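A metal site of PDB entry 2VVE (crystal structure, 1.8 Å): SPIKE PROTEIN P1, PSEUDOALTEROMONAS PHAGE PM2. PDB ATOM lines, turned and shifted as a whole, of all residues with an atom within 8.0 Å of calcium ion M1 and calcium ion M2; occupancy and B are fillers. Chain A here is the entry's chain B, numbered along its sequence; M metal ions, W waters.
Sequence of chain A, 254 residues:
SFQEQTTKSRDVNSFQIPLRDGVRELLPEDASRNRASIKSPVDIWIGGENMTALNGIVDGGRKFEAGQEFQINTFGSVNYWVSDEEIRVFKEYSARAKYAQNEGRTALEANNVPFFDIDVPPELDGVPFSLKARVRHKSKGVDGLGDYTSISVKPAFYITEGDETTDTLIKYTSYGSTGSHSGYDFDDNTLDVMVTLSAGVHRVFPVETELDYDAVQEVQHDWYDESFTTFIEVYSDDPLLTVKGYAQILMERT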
ATOM      1  N   TYR A  99     -15.647  -8.647 -16.359  1.00  0.00           N
ATOM      2  CA  TYR A  99     -17.000  -8.712 -16.911  1.00  0.00           C
ATOM      3  C   TYR A  99     -17.032  -7.932 -18.226  1.00  0.00           C
ATOM      4  O   TYR A  99     -16.602  -6.775 -18.248  1.00  0.00           O
ATOM      5  CB  TYR A  99     -18.000  -8.038 -15.967  1.00  0.00           C
ATOM      6  CG  TYR A  99     -18.172  -8.680 -14.603  1.00  0.00           C
ATOM      7  CD1 TYR A  99     -18.887  -9.871 -14.462  1.00  0.00           C
ATOM      8  CD2 TYR A  99     -17.665  -8.067 -13.459  1.00  0.00           C
ATOM      9  CE1 TYR A  99     -19.062 -10.454 -13.203  1.00  0.00           C
ATOM     10  CE2 TYR A  99     -17.842  -8.622 -12.209  1.00  0.00           C
ATOM     11  CZ  TYR A  99     -18.548  -9.822 -12.089  1.00  0.00           C
ATOM     12  OH  TYR A  99     -18.727 -10.383 -10.850  1.00  0.00           O
ATOM     13  N   ASP A 143     -13.651  -9.638  -2.755  1.00  0.00           N
ATOM     14  CA  ASP A 143     -14.175  -8.261  -2.664  1.00  0.00           C
ATOM     15  C   ASP A 143     -15.142  -8.064  -1.495  1.00  0.00           C
ATOM     16  O   ASP A 143     -15.959  -7.143  -1.497  1.00  0.00           O
ATOM     17  CB  ASP A 143     -14.848  -7.840  -3.977  1.00  0.00           C
ATOM     18  CG  ASP A 143     -13.883  -7.750  -5.136  1.00  0.00           C
ATOM     19  OD1 ASP A 143     -12.665  -7.566  -4.911  1.00  0.00           O
ATOM     20  OD2 ASP A 143     -14.353  -7.860  -6.275  1.00  0.00           O
ATOM     21  N   ALA A 215     -23.746  -9.922  -7.133  1.00  0.00           N
ATOM     22  CA  ALA A 215     -22.457  -9.220  -7.261  1.00  0.00           C
ATOM     23  C   ALA A 215     -22.700  -7.723  -7.378  1.00  0.00           C
ATOM     24  O   ALA A 215     -21.995  -6.914  -6.776  1.00  0.00           O
ATOM     25  CB  ALA A 215     -21.671  -9.733  -8.478  1.00  0.00           C
ATOM     26  N   VAL A 216     -23.715  -7.369  -8.160  1.00  0.00           N
ATOM     27  CA  VAL A 216     -24.089  -5.966  -8.376  1.00  0.00           C
ATOM     28  C   VAL A 216     -24.543  -5.354  -7.051  1.00  0.00           C
ATOM     29  O   VAL A 216     -24.085  -4.272  -6.683  1.00  0.00           O
ATOM     30  CB  VAL A 216     -25.191  -5.835  -9.461  1.00  0.00           C
ATOM     31  CG1 VAL A 216     -25.675  -4.380  -9.585  1.00  0.00           C
ATOM     32  CG2 VAL A 216     -24.691  -6.368 -10.814  1.00  0.00           C
ATOM     33  N   VAL A 219     -21.474  -6.183  -3.800  1.00  0.00           N
ATOM     34  CA  VAL A 219     -20.103  -5.652  -3.974  1.00  0.00           C
ATOM     35  C   VAL A 219     -19.928  -4.653  -5.132  1.00  0.00           C
ATOM     36  O   VAL A 219     -18.801  -4.306  -5.494  1.00  0.00           O
ATOM     37  CB  VAL A 219     -19.029  -6.791  -4.009  1.00  0.00           C
ATOM     38  CG1 VAL A 219     -19.003  -7.535  -2.674  1.00  0.00           C
ATOM     39  CG2 VAL A 219     -19.272  -7.767  -5.174  1.00  0.00           C
ATOM     40  N   GLN A 220     -21.047  -4.159  -5.675  1.00  0.00           N
ATOM     41  CA  GLN A 220     -21.064  -3.087  -6.699  1.00  0.00           C
ATOM     42  C   GLN A 220     -20.271  -3.386  -7.973  1.00  0.00           C
ATOM     43  O   GLN A 220     -19.608  -2.518  -8.546  1.00  0.00           O
ATOM     44  CB  GLN A 220     -20.659  -1.731  -6.077  1.00  0.00           C
ATOM     45  CG  GLN A 220     -21.606  -1.237  -4.965  1.00  0.00           C
ATOM     46  CD  GLN A 220     -21.503  -2.035  -3.683  1.00  0.00           C
ATOM     47  OE1 GLN A 220     -20.410  -2.274  -3.166  1.00  0.00           O
ATOM     48  NE2 GLN A 220     -22.648  -2.479  -3.165  1.00  0.00           N
ATOM     49  N   HIS A 221     -20.333  -4.638  -8.417  1.00  0.00           N
ATOM     50  CA  HIS A 221     -19.666  -5.039  -9.656  1.00  0.00           C
ATOM     51  C   HIS A 221     -20.381  -4.446 -10.863  1.00  0.00           C
ATOM     52  O   HIS A 221     -21.620  -4.347 -10.885  1.00  0.00           O
ATOM     53  CB  HIS A 221     -19.543  -6.561  -9.728  1.00  0.00           C
ATOM     54  CG  HIS A 221     -18.421  -7.111  -8.900  1.00  0.00           C
ATOM     55  ND1 HIS A 221     -18.090  -8.450  -8.885  1.00  0.00           N
ATOM     56  CD2 HIS A 221     -17.558  -6.497  -8.063  1.00  0.00           C
ATOM     57  CE1 HIS A 221     -17.083  -8.646  -8.053  1.00  0.00           C
ATOM     58  NE2 HIS A 221     -16.730  -7.468  -7.551  1.00  0.00           N
ATOM     59  N   ASP A 222     -19.571  -4.031 -11.823  1.00  0.00           N
ATOM     60  CA  ASP A 222     -20.001  -3.360 -13.042  1.00  0.00           C
ATOM     61  C   ASP A 222     -19.287  -4.019 -14.207  1.00  0.00           C
ATOM     62  O   ASP A 222     -18.251  -4.658 -14.012  1.00  0.00           O
ATOM     63  CB  ASP A 222     -19.543  -1.886 -13.036  1.00  0.00           C
ATOM     64  CG  ASP A 222     -20.159  -1.071 -11.917  1.00  0.00           C
ATOM     65  OD1 ASP A 222     -21.340  -0.674 -12.051  1.00  0.00           O
ATOM     66  OD2 ASP A 222     -19.455  -0.790 -10.917  1.00  0.00           O
ATOM     67  N   TRP A 223     -19.812  -3.856 -15.411  1.00  0.00           N
ATOM     68  CA  TRP A 223     -19.054  -4.221 -16.602  1.00  0.00           C
ATOM     69  C   TRP A 223     -17.650  -3.601 -16.560  1.00  0.00           C
ATOM     70  O   TRP A 223     -17.469  -2.447 -16.119  1.00  0.00           O
ATOM     71  CB  TRP A 223     -19.819  -3.849 -17.872  1.00  0.00           C
ATOM     72  CG  TRP A 223     -21.148  -4.545 -17.931  1.00  0.00           C
ATOM     73  CD1 TRP A 223     -22.380  -3.975 -17.787  1.00  0.00           C
ATOM     74  CD2 TRP A 223     -21.369  -5.943 -18.113  1.00  0.00           C
ATOM     75  NE1 TRP A 223     -23.360  -4.940 -17.883  1.00  0.00           N
ATOM     76  CE2 TRP A 223     -22.764  -6.156 -18.075  1.00  0.00           C
ATOM     77  CE3 TRP A 223     -20.521  -7.041 -18.311  1.00  0.00           C
ATOM     78  CZ2 TRP A 223     -23.334  -7.435 -18.225  1.00  0.00           C
ATOM     79  CZ3 TRP A 223     -21.085  -8.314 -18.465  1.00  0.00           C
ATOM     80  CH2 TRP A 223     -22.479  -8.498 -18.411  1.00  0.00           C
ATOM     81  N   TYR A 224     -16.673  -4.391 -16.976  1.00  0.00           N
ATOM     82  CA  TYR A 224     -15.232  -4.049 -16.947  1.00  0.00           C
ATOM     83  C   TYR A 224     -14.578  -4.123 -15.566  1.00  0.00           C
ATOM     84  O   TYR A 224     -13.363  -3.961 -15.443  1.00  0.00           O
ATOM     85  CB  TYR A 224     -14.935  -2.709 -17.636  1.00  0.00           C
ATOM     86  CG  TYR A 224     -15.473  -2.631 -19.044  1.00  0.00           C
ATOM     87  CD1 TYR A 224     -14.963  -3.450 -20.055  1.00  0.00           C
ATOM     88  CD2 TYR A 224     -16.514  -1.748 -19.360  1.00  0.00           C
ATOM     89  CE1 TYR A 224     -15.461  -3.385 -21.355  1.00  0.00           C
ATOM     90  CE2 TYR A 224     -17.017  -1.675 -20.655  1.00  0.00           C
ATOM     91  CZ  TYR A 224     -16.488  -2.497 -21.643  1.00  0.00           C
ATOM     92  OH  TYR A 224     -16.978  -2.426 -22.923  1.00  0.00           O
ATOM     93  N   ASP A 225     -15.381  -4.375 -14.527  1.00  0.00           N
ATOM     94  CA  ASP A 225     -14.822  -4.700 -13.204  1.00  0.00           C
ATOM     95  C   ASP A 225     -14.216  -6.103 -13.234  1.00  0.00           C
ATOM     96  O   ASP A 225     -14.478  -6.881 -14.155  1.00  0.00           O
ATOM     97  CB  ASP A 225     -15.887  -4.617 -12.111  1.00  0.00           C
ATOM     98  CG  ASP A 225     -16.094  -3.209 -11.577  1.00  0.00           C
ATOM     99  OD1 ASP A 225     -15.220  -2.336 -11.766  1.00  0.00           O
ATOM    100  OD2 ASP A 225     -17.138  -2.973 -10.943  1.00  0.00           O
ATOM    101  N   GLU A 226     -13.394  -6.420 -12.231  1.00  0.00           N
ATOM    102  CA  GLU A 226     -12.895  -7.770 -12.030  1.00  0.00           C
ATOM    103  C   GLU A 226     -14.023  -8.696 -11.545  1.00  0.00           C
ATOM    104  O   GLU A 226     -14.695  -8.388 -10.556  1.00  0.00           O
ATOM    105  CB  GLU A 226     -11.759  -7.778 -10.995  1.00  0.00           C
ATOM    106  CG  GLU A 226     -10.393  -7.405 -11.554  1.00  0.00           C
ATOM    107  CD  GLU A 226      -9.301  -7.398 -10.497  1.00  0.00           C
ATOM    108  OE1 GLU A 226      -9.596  -7.098  -9.321  1.00  0.00           O
ATOM    109  OE2 GLU A 226      -8.139  -7.694 -10.859  1.00  0.00           O
HETATM  110 CA    CA M   1     -17.718  -1.318  -9.331  1.00  0.00          CA
HETATM  111 CA    CA M   2     -21.236   0.299  -9.627  1.00  0.00          CA
HETATM  112  O   HOH W   1     -18.956   0.460  -8.093  1.00  0.00           O
HETATM  113  O   HOH W   2     -22.731  -1.766  -9.499  1.00  0.00           O
HETATM  114  O   HOH W   3     -17.272  -2.968  -7.321  1.00  0.00           O
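OD2 of Asp 222 binds calcium ion M2 (2.5 Å). Water W2 binds calcium ion M2 (2.6 Å). Calcium ion M2 is bound by OD1 of Asp 222 (2.6 Å). Calcium ion M2 is bound by water W1 (2.8 Å). Calcium ion M2 has four donor atoms within binding distance.
O of Asp 225 lies within hydrogen-bond range of N of Tyr 99. N of Gln 220 is in hydrogen-bond range of O of Ala 215, 3.1 Å away.
Of the 12 residues printed, 3 come within 4 Å of calcium ion M1. The nearest printed residue that does not touch calcium ion M1 is His 221 (4.2 Å).
Calcium ion M1 is bound by O of Gln 220, OD2 of Asp 225, OD2 of Asp 222, water W1 and water W3.
Within 4 Å of calcium ion M2: Gln 220 and Asp 222.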
